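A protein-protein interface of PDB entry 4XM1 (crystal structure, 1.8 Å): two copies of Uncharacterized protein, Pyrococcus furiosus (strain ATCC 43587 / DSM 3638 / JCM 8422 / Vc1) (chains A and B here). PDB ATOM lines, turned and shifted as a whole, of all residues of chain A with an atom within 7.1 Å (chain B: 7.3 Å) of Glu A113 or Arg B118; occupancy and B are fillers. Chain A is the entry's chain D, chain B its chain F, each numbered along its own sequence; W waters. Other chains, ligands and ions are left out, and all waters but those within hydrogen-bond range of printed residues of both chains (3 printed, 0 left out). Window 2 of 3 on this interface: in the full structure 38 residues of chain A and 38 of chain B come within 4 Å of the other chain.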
ATOM      1  N   THR A  68     -12.921 -19.565 -13.855  1.00  0.00           N
ATOM      2  CA  THR A  68     -12.160 -19.968 -14.982  1.00  0.00           C
ATOM      3  C   THR A  68     -13.029 -20.575 -16.078  1.00  0.00           C
ATOM      4  O   THR A  68     -14.230 -20.815 -15.892  1.00  0.00           O
ATOM      5  CB  THR A  68     -11.046 -20.983 -14.621  1.00  0.00           C
ATOM      6  OG1 THR A  68     -11.616 -22.262 -14.433  1.00  0.00           O
ATOM      7  CG2 THR A  68     -10.276 -20.595 -13.263  1.00  0.00           C
ATOM      8  N   TYR A  71     -10.787 -24.876 -19.506  1.00  0.00           N
ATOM      9  CA  TYR A  71      -9.934 -25.140 -20.659  1.00  0.00           C
ATOM     10  C   TYR A  71      -9.162 -26.462 -20.557  1.00  0.00           C
ATOM     11  O   TYR A  71      -8.873 -27.102 -21.561  1.00  0.00           O
ATOM     12  CB  TYR A  71      -8.962 -23.967 -20.756  1.00  0.00           C
ATOM     13  CG  TYR A  71      -7.929 -23.978 -21.876  1.00  0.00           C
ATOM     14  CD1 TYR A  71      -8.132 -23.163 -22.980  1.00  0.00           C
ATOM     15  CD2 TYR A  71      -6.744 -24.729 -21.785  1.00  0.00           C
ATOM     16  CE1 TYR A  71      -7.185 -23.048 -24.015  1.00  0.00           C
ATOM     17  CE2 TYR A  71      -5.744 -24.658 -22.888  1.00  0.00           C
ATOM     18  CZ  TYR A  71      -6.035 -23.845 -23.977  1.00  0.00           C
ATOM     19  OH  TYR A  71      -5.092 -23.733 -24.980  1.00  0.00           O
ATOM     20  N   MET A  72      -8.833 -26.893 -19.331  1.00  0.00           N
ATOM     21  CA  MET A  72      -7.868 -28.007 -19.207  1.00  0.00           C
ATOM     22  C   MET A  72      -8.516 -29.412 -19.045  1.00  0.00           C
ATOM     23  O   MET A  72      -7.813 -30.450 -19.046  1.00  0.00           O
ATOM     24  CB  MET A  72      -6.869 -27.767 -18.072  1.00  0.00           C
ATOM     25  CG  MET A  72      -5.755 -26.760 -18.311  1.00  0.00           C
ATOM     26  SD  MET A  72      -4.746 -26.916 -19.807  1.00  0.00           S
ATOM     27  CE  MET A  72      -3.876 -25.275 -19.598  1.00  0.00           C
ATOM     28  N   TYR A 109     -10.539 -16.485 -16.690  1.00  0.00           N
ATOM     29  CA  TYR A 109      -9.087 -16.823 -16.377  1.00  0.00           C
ATOM     30  C   TYR A 109      -8.925 -18.290 -16.882  1.00  0.00           C
ATOM     31  O   TYR A 109      -9.880 -19.067 -16.777  1.00  0.00           O
ATOM     32  CB  TYR A 109      -8.747 -16.649 -14.831  1.00  0.00           C
ATOM     33  CG  TYR A 109      -8.688 -15.175 -14.478  1.00  0.00           C
ATOM     34  CD1 TYR A 109      -7.602 -14.369 -14.922  1.00  0.00           C
ATOM     35  CD2 TYR A 109      -9.780 -14.550 -13.855  1.00  0.00           C
ATOM     36  CE1 TYR A 109      -7.576 -12.964 -14.710  1.00  0.00           C
ATOM     37  CE2 TYR A 109      -9.773 -13.157 -13.597  1.00  0.00           C
ATOM     38  CZ  TYR A 109      -8.692 -12.380 -14.025  1.00  0.00           C
ATOM     39  OH  TYR A 109      -8.652 -11.069 -13.793  1.00  0.00           O
ATOM     40  N   ARG A 110      -7.826 -18.610 -17.620  1.00  0.00           N
ATOM     41  CA  ARG A 110      -7.605 -20.000 -18.052  1.00  0.00           C
ATOM     42  C   ARG A 110      -7.520 -20.974 -16.803  1.00  0.00           C
ATOM     43  O   ARG A 110      -6.796 -20.715 -15.836  1.00  0.00           O
ATOM     44  CB  ARG A 110      -6.393 -20.075 -19.005  1.00  0.00           C
ATOM     45  CG  ARG A 110      -6.154 -21.494 -19.475  1.00  0.00           C
ATOM     46  CD  ARG A 110      -5.217 -21.473 -20.632  1.00  0.00           C
ATOM     47  NE  ARG A 110      -5.698 -20.595 -21.679  1.00  0.00           N
ATOM     48  CZ  ARG A 110      -4.890 -20.316 -22.719  1.00  0.00           C
ATOM     49  NH1 ARG A 110      -3.673 -20.850 -22.715  1.00  0.00           N
ATOM     50  NH2 ARG A 110      -5.249 -19.494 -23.690  1.00  0.00           N
ATOM     51  N   ASP A 111      -8.322 -22.050 -16.822  1.00  0.00           N
ATOM     52  CA  ASP A 111      -8.188 -23.276 -16.056  1.00  0.00           C
ATOM     53  C   ASP A 111      -6.703 -23.620 -15.766  1.00  0.00           C
ATOM     54  O   ASP A 111      -5.868 -23.669 -16.659  1.00  0.00           O
ATOM     55  CB  ASP A 111      -8.800 -24.419 -16.939  1.00  0.00           C
ATOM     56  CG  ASP A 111      -9.114 -25.664 -16.206  1.00  0.00           C
ATOM     57  OD1 ASP A 111      -8.804 -25.772 -14.976  1.00  0.00           O
ATOM     58  OD2 ASP A 111      -9.666 -26.600 -16.887  1.00  0.00           O
ATOM     59  N   THR A 112      -6.371 -23.854 -14.520  1.00  0.00           N
ATOM     60  CA  THR A 112      -5.011 -24.022 -14.068  1.00  0.00           C
ATOM     61  C   THR A 112      -4.170 -22.770 -13.872  1.00  0.00           C
ATOM     62  O   THR A 112      -3.137 -22.881 -13.131  1.00  0.00           O
ATOM     63  CB  THR A 112      -4.180 -25.192 -14.701  1.00  0.00           C
ATOM     64  OG1 THR A 112      -3.696 -24.798 -16.022  1.00  0.00           O
ATOM     65  CG2 THR A 112      -5.059 -26.531 -14.699  1.00  0.00           C
ATOM     66  N   GLU A 113      -4.647 -21.617 -14.386  1.00  0.00           N
ATOM     67  CA  GLU A 113      -3.967 -20.360 -14.373  1.00  0.00           C
ATOM     68  C   GLU A 113      -4.699 -19.236 -13.680  1.00  0.00           C
ATOM     69  O   GLU A 113      -4.401 -18.103 -13.938  1.00  0.00           O
ATOM     70  CB  GLU A 113      -3.593 -20.030 -15.896  1.00  0.00           C
ATOM     71  CG  GLU A 113      -3.026 -21.229 -16.403  1.00  0.00           C
ATOM     72  CD  GLU A 113      -2.592 -21.016 -17.895  1.00  0.00           C
ATOM     73  OE1 GLU A 113      -1.929 -21.919 -18.467  1.00  0.00           O
ATOM     74  OE2 GLU A 113      -2.965 -19.927 -18.369  1.00  0.00           O
ATOM     75  N   LEU A 114      -5.531 -19.535 -12.641  1.00  0.00           N
ATOM     76  CA  LEU A 114      -6.234 -18.419 -11.983  1.00  0.00           C
ATOM     77  C   LEU A 114      -5.238 -17.655 -11.109  1.00  0.00           C
ATOM     78  O   LEU A 114      -4.672 -18.313 -10.204  1.00  0.00           O
ATOM     79  CB  LEU A 114      -7.411 -18.953 -11.144  1.00  0.00           C
ATOM     80  CG  LEU A 114      -8.112 -17.863 -10.287  1.00  0.00           C
ATOM     81  CD1 LEU A 114      -8.943 -16.830 -10.967  1.00  0.00           C
ATOM     82  CD2 LEU A 114      -8.999 -18.512  -9.046  1.00  0.00           C
ATOM     83  N   PRO A 115      -5.094 -16.334 -11.286  1.00  0.00           N
ATOM     84  CA  PRO A 115      -4.049 -15.663 -10.558  1.00  0.00           C
ATOM     85  C   PRO A 115      -4.484 -15.557  -9.080  1.00  0.00           C
ATOM     86  O   PRO A 115      -5.703 -15.644  -8.808  1.00  0.00           O
ATOM     87  CB  PRO A 115      -4.078 -14.259 -11.160  1.00  0.00           C
ATOM     88  CG  PRO A 115      -4.353 -14.685 -12.844  1.00  0.00           C
ATOM     89  CD  PRO A 115      -5.416 -15.680 -12.626  1.00  0.00           C
ATOM     90  N   TYR A 116      -3.523 -15.325  -8.216  1.00  0.00           N
ATOM     91  CA  TYR A 116      -3.917 -14.923  -6.828  1.00  0.00           C
ATOM     92  C   TYR A 116      -3.425 -13.546  -6.654  1.00  0.00           C
ATOM     93  O   TYR A 116      -2.223 -13.296  -6.305  1.00  0.00           O
ATOM     94  CB  TYR A 116      -3.345 -15.871  -5.851  1.00  0.00           C
ATOM     95  CG  TYR A 116      -3.670 -15.395  -4.453  1.00  0.00           C
ATOM     96  CD1 TYR A 116      -2.718 -14.768  -3.677  1.00  0.00           C
ATOM     97  CD2 TYR A 116      -4.917 -15.615  -3.952  1.00  0.00           C
ATOM     98  CE1 TYR A 116      -3.055 -14.349  -2.313  1.00  0.00           C
ATOM     99  CE2 TYR A 116      -5.262 -15.203  -2.680  1.00  0.00           C
ATOM    100  CZ  TYR A 116      -4.317 -14.552  -1.876  1.00  0.00           C
ATOM    101  OH  TYR A 116      -4.603 -14.183  -0.541  1.00  0.00           O
ATOM    102  N   VAL A 120      -7.597  -9.902  -9.537  1.00  0.00           N
ATOM    103  CA  VAL A 120      -8.732 -10.840  -9.523  1.00  0.00           C
ATOM    104  C   VAL A 120      -9.692 -10.384  -8.417  1.00  0.00           C
ATOM    105  O   VAL A 120     -10.942 -10.354  -8.631  1.00  0.00           O
ATOM    106  CB  VAL A 120      -8.335 -12.352  -9.414  1.00  0.00           C
ATOM    107  CG1 VAL A 120      -9.613 -13.274  -9.391  1.00  0.00           C
ATOM    108  CG2 VAL A 120      -7.378 -12.775 -10.473  1.00  0.00           C
ATOM    109  N   HIS A 148      -5.886 -28.464  -5.817  1.00  0.00           N
ATOM    110  CA  HIS A 148      -6.058 -27.669  -7.054  1.00  0.00           C
ATOM    111  C   HIS A 148      -5.845 -26.197  -6.657  1.00  0.00           C
ATOM    112  O   HIS A 148      -6.664 -25.674  -5.874  1.00  0.00           O
ATOM    113  CB  HIS A 148      -7.456 -27.859  -7.667  1.00  0.00           C
ATOM    114  CG  HIS A 148      -7.506 -27.566  -9.157  1.00  0.00           C
ATOM    115  ND1 HIS A 148      -6.905 -26.453  -9.719  1.00  0.00           N
ATOM    116  CD2 HIS A 148      -8.050 -28.261 -10.190  1.00  0.00           C
ATOM    117  CE1 HIS A 148      -7.093 -26.457 -11.035  1.00  0.00           C
ATOM    118  NE2 HIS A 148      -7.810 -27.529 -11.340  1.00  0.00           N
ATOM    119  N   PRO A 149      -4.807 -25.537  -7.193  1.00  0.00           N
ATOM    120  CA  PRO A 149      -4.587 -24.100  -6.865  1.00  0.00           C
ATOM    121  C   PRO A 149      -5.826 -23.274  -7.217  1.00  0.00           C
ATOM    122  O   PRO A 149      -6.107 -22.300  -6.551  1.00  0.00           O
ATOM    123  CB  PRO A 149      -3.422 -23.693  -7.777  1.00  0.00           C
ATOM    124  CG  PRO A 149      -3.365 -24.739  -8.815  1.00  0.00           C
ATOM    125  CD  PRO A 149      -3.805 -25.997  -8.177  1.00  0.00           C
ATOM    126  N   ASP A 150      -6.538 -23.609  -8.318  1.00  0.00           N
ATOM    127  CA  ASP A 150      -7.692 -22.797  -8.729  1.00  0.00           C
ATOM    128  C   ASP A 150      -8.768 -22.841  -7.600  1.00  0.00           C
ATOM    129  O   ASP A 150      -9.435 -21.806  -7.385  1.00  0.00           O
ATOM    130  CB  ASP A 150      -8.326 -23.369  -9.982  1.00  0.00           C
ATOM    131  CG  ASP A 150      -7.560 -23.067 -11.249  1.00  0.00           C
ATOM    132  OD1 ASP A 150      -7.988 -23.619 -12.294  1.00  0.00           O
ATOM    133  OD2 ASP A 150      -6.605 -22.255 -11.294  1.00  0.00           O
ATOM    134  N   ARG A 153      -7.503 -20.770  -4.380  1.00  0.00           N
ATOM    135  CA  ARG A 153      -7.514 -19.339  -4.601  1.00  0.00           C
ATOM    136  C   ARG A 153      -8.901 -18.697  -4.775  1.00  0.00           C
ATOM    137  O   ARG A 153      -8.959 -17.561  -4.460  1.00  0.00           O
ATOM    138  CB  ARG A 153      -6.681 -18.989  -5.914  1.00  0.00           C
ATOM    139  CG  ARG A 153      -5.083 -19.272  -5.755  1.00  0.00           C
ATOM    140  CD  ARG A 153      -4.329 -19.313  -7.128  1.00  0.00           C
ATOM    141  NE  ARG A 153      -2.899 -19.425  -6.778  1.00  0.00           N
ATOM    142  CZ  ARG A 153      -1.890 -18.994  -7.528  1.00  0.00           C
ATOM    143  NH1 ARG A 153      -2.118 -18.590  -8.791  1.00  0.00           N
ATOM    144  NH2 ARG A 153      -0.657 -19.085  -7.026  1.00  0.00           N
ATOM    145  N   PRO B 115      10.231 -20.756  -7.608  1.00  0.00           N
ATOM    146  CA  PRO B 115       8.966 -20.107  -7.987  1.00  0.00           C
ATOM    147  C   PRO B 115       7.798 -21.059  -7.837  1.00  0.00           C
ATOM    148  O   PRO B 115       7.926 -22.303  -8.007  1.00  0.00           O
ATOM    149  CB  PRO B 115       9.169 -19.816  -9.534  1.00  0.00           C
ATOM    150  CG  PRO B 115      10.700 -19.829  -9.632  1.00  0.00           C
ATOM    151  CD  PRO B 115      11.056 -20.983  -8.787  1.00  0.00           C
ATOM    152  N   TYR B 116       6.616 -20.511  -7.555  1.00  0.00           N
ATOM    153  CA  TYR B 116       5.418 -21.306  -7.540  1.00  0.00           C
ATOM    154  C   TYR B 116       4.621 -20.796  -8.726  1.00  0.00           C
ATOM    155  O   TYR B 116       3.930 -19.775  -8.653  1.00  0.00           O
ATOM    156  CB  TYR B 116       4.609 -21.210  -6.179  1.00  0.00           C
ATOM    157  CG  TYR B 116       3.330 -22.005  -6.225  1.00  0.00           C
ATOM    158  CD1 TYR B 116       2.076 -21.367  -6.468  1.00  0.00           C
ATOM    159  CD2 TYR B 116       3.341 -23.405  -6.102  1.00  0.00           C
ATOM    160  CE1 TYR B 116       0.898 -22.120  -6.512  1.00  0.00           C
ATOM    161  CE2 TYR B 116       2.199 -24.182  -6.197  1.00  0.00           C
ATOM    162  CZ  TYR B 116       0.952 -23.516  -6.412  1.00  0.00           C
ATOM    163  OH  TYR B 116      -0.159 -24.204  -6.478  1.00  0.00           O
ATOM    164  N   SER B 117       4.865 -21.440  -9.871  1.00  0.00           N
ATOM    165  CA  SER B 117       4.326 -20.952 -11.124  1.00  0.00           C
ATOM    166  C   SER B 117       4.036 -22.054 -12.153  1.00  0.00           C
ATOM    167  O   SER B 117       4.552 -23.210 -12.047  1.00  0.00           O
ATOM    168  CB  SER B 117       5.347 -20.001 -11.773  1.00  0.00           C
ATOM    169  OG  SER B 117       6.566 -20.697 -11.990  1.00  0.00           O
ATOM    170  N   ARG B 118       3.375 -21.668 -13.239  1.00  0.00           N
ATOM    171  CA  ARG B 118       3.091 -22.669 -14.277  1.00  0.00           C
ATOM    172  C   ARG B 118       4.419 -23.159 -14.860  1.00  0.00           C
ATOM    173  O   ARG B 118       4.594 -24.337 -15.107  1.00  0.00           O
ATOM    174  CB  ARG B 118       2.166 -22.096 -15.346  1.00  0.00           C
ATOM    175  CG  ARG B 118       2.106 -22.903 -16.659  1.00  0.00           C
ATOM    176  CD  ARG B 118       1.262 -22.076 -17.548  1.00  0.00           C
ATOM    177  NE  ARG B 118       2.011 -20.868 -17.898  1.00  0.00           N
ATOM    178  CZ  ARG B 118       1.569 -19.760 -18.506  1.00  0.00           C
ATOM    179  NH1 ARG B 118       0.296 -19.575 -18.911  1.00  0.00           N
ATOM    180  NH2 ARG B 118       2.448 -18.775 -18.687  1.00  0.00           N
ATOM    181  N   GLU B 119       5.360 -22.253 -15.012  1.00  0.00           N
ATOM    182  CA  GLU B 119       6.662 -22.554 -15.595  1.00  0.00           C
ATOM    183  C   GLU B 119       7.358 -23.717 -14.886  1.00  0.00           C
ATOM    184  O   GLU B 119       7.947 -24.592 -15.539  1.00  0.00           O
ATOM    185  CB  GLU B 119       7.565 -21.314 -15.679  1.00  0.00           C
ATOM    186  CG  GLU B 119       9.055 -21.617 -16.073  1.00  0.00           C
ATOM    187  CD  GLU B 119       9.970 -20.337 -16.064  1.00  0.00           C
ATOM    188  OE1 GLU B 119       9.701 -19.357 -15.281  1.00  0.00           O
ATOM    189  OE2 GLU B 119      10.924 -20.300 -16.886  1.00  0.00           O
ATOM    190  N   VAL B 120       7.341 -23.719 -13.540  1.00  0.00           N
ATOM    191  CA  VAL B 120       7.992 -24.823 -12.854  1.00  0.00           C
ATOM    192  C   VAL B 120       7.169 -26.144 -13.087  1.00  0.00           C
ATOM    193  O   VAL B 120       7.734 -27.230 -13.379  1.00  0.00           O
ATOM    194  CB  VAL B 120       8.221 -24.513 -11.341  1.00  0.00           C
ATOM    195  CG1 VAL B 120       9.041 -25.641 -10.659  1.00  0.00           C
ATOM    196  CG2 VAL B 120       9.024 -23.226 -11.131  1.00  0.00           C
ATOM    197  N   ARG B 121       5.831 -26.050 -13.006  1.00  0.00           N
ATOM    198  CA  ARG B 121       4.973 -27.225 -13.226  1.00  0.00           C
ATOM    199  C   ARG B 121       5.396 -27.806 -14.644  1.00  0.00           C
ATOM    200  O   ARG B 121       5.473 -29.038 -14.826  1.00  0.00           O
ATOM    201  CB  ARG B 121       3.489 -26.898 -13.164  1.00  0.00           C
ATOM    202  CG  ARG B 121       2.888 -26.507 -11.714  1.00  0.00           C
ATOM    203  CD  ARG B 121       1.313 -26.349 -11.773  1.00  0.00           C
ATOM    204  NE  ARG B 121       0.924 -25.680 -10.510  1.00  0.00           N
ATOM    205  CZ  ARG B 121       0.754 -24.353 -10.413  1.00  0.00           C
ATOM    206  NH1 ARG B 121       0.821 -23.580 -11.503  1.00  0.00           N
ATOM    207  NH2 ARG B 121       0.460 -23.821  -9.205  1.00  0.00           N
ATOM    208  N   LYS B 122       5.748 -26.922 -15.555  1.00  0.00           N
ATOM    209  CA  LYS B 122       6.040 -27.354 -16.935  1.00  0.00           C
ATOM    210  C   LYS B 122       7.309 -28.237 -16.934  1.00  0.00           C
ATOM    211  O   LYS B 122       7.401 -29.221 -17.703  1.00  0.00           O
ATOM    212  CB  LYS B 122       6.184 -26.158 -17.875  1.00  0.00           C
ATOM    213  CG  LYS B 122       4.877 -25.696 -18.537  1.00  0.00           C
ATOM    214  CD  LYS B 122       5.191 -24.497 -19.384  1.00  0.00           C
ATOM    215  CE  LYS B 122       3.908 -24.006 -19.961  1.00  0.00           C
ATOM    216  NZ  LYS B 122       4.100 -22.625 -20.503  1.00  0.00           N
ATOM    217  N   ASP B 123       8.265 -27.892 -16.069  1.00  0.00           N
ATOM    218  CA  ASP B 123       9.531 -28.649 -15.909  1.00  0.00           C
ATOM    219  C   ASP B 123       9.274 -30.057 -15.370  1.00  0.00           C
ATOM    220  O   ASP B 123       9.846 -31.050 -15.871  1.00  0.00           O
ATOM    221  CB  ASP B 123      10.515 -27.928 -14.959  1.00  0.00           C
ATOM    222  CG  ASP B 123      11.064 -26.632 -15.545  1.00  0.00           C
ATOM    223  OD1 ASP B 123      11.191 -26.540 -16.784  1.00  0.00           O
ATOM    224  OD2 ASP B 123      11.320 -25.694 -14.763  1.00  0.00           O
ATOM    225  N   LEU B 124       8.461 -30.136 -14.305  1.00  0.00           N
ATOM    226  CA  LEU B 124       8.070 -31.381 -13.749  1.00  0.00           C
ATOM    227  C   LEU B 124       7.312 -32.255 -14.691  1.00  0.00           C
ATOM    228  O   LEU B 124       7.604 -33.478 -14.815  1.00  0.00           O
ATOM    229  CB  LEU B 124       7.349 -31.215 -12.392  1.00  0.00           C
ATOM    230  CG  LEU B 124       8.169 -30.508 -11.352  1.00  0.00           C
ATOM    231  CD1 LEU B 124       7.295 -30.357 -10.050  1.00  0.00           C
ATOM    232  CD2 LEU B 124       9.536 -31.200 -11.074  1.00  0.00           C
ATOM    233  N   VAL B 125       6.414 -31.632 -15.426  1.00  0.00           N
ATOM    234  CA  VAL B 125       5.492 -32.321 -16.269  1.00  0.00           C
ATOM    235  C   VAL B 125       6.297 -32.867 -17.489  1.00  0.00           C
ATOM    236  O   VAL B 125       6.055 -33.988 -17.931  1.00  0.00           O
ATOM    237  CB  VAL B 125       4.398 -31.372 -16.683  1.00  0.00           C
ATOM    238  CG1 VAL B 125       3.805 -31.783 -17.959  1.00  0.00           C
ATOM    239  CG2 VAL B 125       3.344 -31.306 -15.614  1.00  0.00           C
ATOM    240  N   LEU B 157       3.685 -28.324  -6.004  1.00  0.00           N
ATOM    241  CA  LEU B 157       3.997 -28.399  -7.450  1.00  0.00           C
ATOM    242  C   LEU B 157       4.125 -29.849  -7.990  1.00  0.00           C
ATOM    243  O   LEU B 157       3.787 -30.133  -9.141  1.00  0.00           O
ATOM    244  CB  LEU B 157       5.293 -27.633  -7.711  1.00  0.00           C
ATOM    245  CG  LEU B 157       5.269 -26.072  -7.661  1.00  0.00           C
ATOM    246  CD1 LEU B 157       6.711 -25.569  -7.638  1.00  0.00           C
ATOM    247  CD2 LEU B 157       4.405 -25.470  -8.839  1.00  0.00           C
ATOM    248  N   SER B 161       1.754 -31.317 -10.732  1.00  0.00           N
ATOM    249  CA  SER B 161       2.348 -31.629 -12.040  1.00  0.00           C
ATOM    250  C   SER B 161       2.009 -33.093 -12.306  1.00  0.00           C
ATOM    251  O   SER B 161       1.876 -33.501 -13.434  1.00  0.00           O
ATOM    252  CB  SER B 161       3.830 -31.462 -11.953  1.00  0.00           C
ATOM    253  OG  SER B 161       4.117 -30.111 -11.578  1.00  0.00           O
ATOM    254  N   PHE B 164      -1.404 -32.863 -13.649  1.00  0.00           N
ATOM    255  CA  PHE B 164      -1.515 -32.161 -14.967  1.00  0.00           C
ATOM    256  C   PHE B 164      -0.769 -32.875 -16.069  1.00  0.00           C
ATOM    257  O   PHE B 164      -1.006 -32.597 -17.255  1.00  0.00           O
ATOM    258  CB  PHE B 164      -1.047 -30.686 -14.944  1.00  0.00           C
ATOM    259  CG  PHE B 164      -1.835 -29.789 -13.968  1.00  0.00           C
ATOM    260  CD1 PHE B 164      -3.112 -30.155 -13.523  1.00  0.00           C
ATOM    261  CD2 PHE B 164      -1.246 -28.628 -13.449  1.00  0.00           C
ATOM    262  CE1 PHE B 164      -3.805 -29.370 -12.580  1.00  0.00           C
ATOM    263  CE2 PHE B 164      -1.965 -27.792 -12.521  1.00  0.00           C
ATOM    264  CZ  PHE B 164      -3.214 -28.165 -12.084  1.00  0.00           C
ATOM    265  N   ASN B 169      -3.826 -30.597 -23.007  1.00  0.00           N
ATOM    266  CA  ASN B 169      -3.840 -29.126 -23.147  1.00  0.00           C
ATOM    267  C   ASN B 169      -2.972 -28.418 -22.135  1.00  0.00           C
ATOM    268  O   ASN B 169      -2.746 -27.212 -22.247  1.00  0.00           O
ATOM    269  CB  ASN B 169      -5.273 -28.582 -23.059  1.00  0.00           C
ATOM    270  CG  ASN B 169      -6.091 -28.950 -24.278  1.00  0.00           C
ATOM    271  OD1 ASN B 169      -5.572 -28.989 -25.390  1.00  0.00           O
ATOM    272  ND2 ASN B 169      -7.360 -29.166 -24.093  1.00  0.00           N
ATOM    273  N   PHE B 170      -2.481 -29.145 -21.144  1.00  0.00           N
ATOM    274  CA  PHE B 170      -1.447 -28.579 -20.306  1.00  0.00           C
ATOM    275  C   PHE B 170      -0.028 -28.751 -20.901  1.00  0.00           C
ATOM    276  O   PHE B 170       0.512 -29.923 -21.067  1.00  0.00           O
ATOM    277  CB  PHE B 170      -1.550 -29.159 -18.877  1.00  0.00           C
ATOM    278  CG  PHE B 170      -0.701 -28.437 -17.899  1.00  0.00           C
ATOM    279  CD1 PHE B 170      -1.255 -27.471 -17.056  1.00  0.00           C
ATOM    280  CD2 PHE B 170       0.641 -28.750 -17.773  1.00  0.00           C
ATOM    281  CE1 PHE B 170      -0.462 -26.809 -16.110  1.00  0.00           C
ATOM    282  CE2 PHE B 170       1.436 -28.106 -16.834  1.00  0.00           C
ATOM    283  CZ  PHE B 170       0.883 -27.119 -16.034  1.00  0.00           C
ATOM    284  N   SER B 171       0.595 -27.603 -21.188  1.00  0.00           N
ATOM    285  CA  SER B 171       1.925 -27.556 -21.741  1.00  0.00           C
ATOM    286  C   SER B 171       1.902 -28.325 -23.046  1.00  0.00           C
ATOM    287  O   SER B 171       2.577 -29.355 -23.179  1.00  0.00           O
ATOM    288  CB  SER B 171       2.924 -28.154 -20.764  1.00  0.00           C
ATOM    289  OG  SER B 171       4.216 -27.686 -21.013  1.00  0.00           O
HETATM  290  O   HOH W   1       1.495 -18.889  -8.960  1.00  0.00           O
HETATM  291  O   HOH W   2      -6.259 -31.247 -21.178  1.00  0.00           O
HETATM  292  O   HOH W   3      -0.651 -23.951 -14.321  1.00  0.00           O
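SD of Met A72 sits at hydrogen-bond distance from N of Phe B170.
NH1 of Arg B118 lies within salt-bridge range of OE1 of Glu A113, 3.3 Å away.
The side-chain sulfur (SD) of Met A72 lies close to the backbone carbonyl oxygen (O) of Asn B169 (3.2 Å).
The side-chain hydroxyl (OH) of Tyr B116 lies within hydrogen-bond range of the guanidinium group (NH2) of Arg B121.
N of Met A72 is in hydrogen-bond range of OD2 of Asp A111 (2.6 Å).
OD1 of Asp A150 lies within hydrogen-bond range of N of Thr A112 (2.8 Å).
O of Leu A114 sits at hydrogen-bond distance from NH1 of Arg A153.
The side-chain carboxylate (OD2) of Asp A111 lies close to the backbone NH (N) of Tyr A71 (3.3 Å).
Among the printed residues, pairs that only touch across the chains: Tyr A71 with Asn B169, Thr A112 with Phe B164, Thr A112 with Phe B170, Pro A149 with Tyr B116, Pro A149 with Arg B121 and Arg A153 with Tyr B116.
Of the printed residues of chain B, Glu A113 touches Arg B118 (3.3 Å).
Printed residues of chain B within 4 Å of Met A72: Asn B169 and Phe B170.
Of the printed residues of chain A, Tyr B116 touches Pro A149 and Arg A153.
Printed residues of chain A within 4 Å of Phe B170: Met A72 (3.4 Å) and Thr A112 (3.8 Å).
Printed residues of chain B within 4 Å of Tyr A71: Asn B169 (3.6 Å).
Of the printed residues of chain A, Asn B169 touches Tyr A71 (3.6 Å) and Met A72 (3.2 Å).
Of the 17 printed residues of chain B, 6 touch a printed residue of chain A.
Printed residues of chain B that touch a printed residue of chain A: Tyr B116, Arg B118, Arg B121, Phe B164, Asn B169 and Phe B170.
Hydrophobic or aromatic side chains of chain B within 4 Å of the printed part of chain A: Tyr B116, Phe B164 and Phe B170.
Hydrophobic or aromatic side chains of chain A that line the printed part of chain B: Tyr A71, Met A72 and Pro A149.
Positions printed for both chains: 115, 116 and 120.
Of the 9 pairs that touch across the chains among the printed residues, none has its exchanged pair printed and touching as well.
Water W1 bridges the backbone carbonyl oxygen of Tyr B116 (2.6 Å) and the guanidinium group of Arg A153 (2.9 Å).
Water W2 bridges O of Met A72 and N of Asn B169.
Water W3 lies within hydrogen-bond range of O of Thr A112 (3.0 Å) and NH1 of Arg B121 (3.2 Å).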
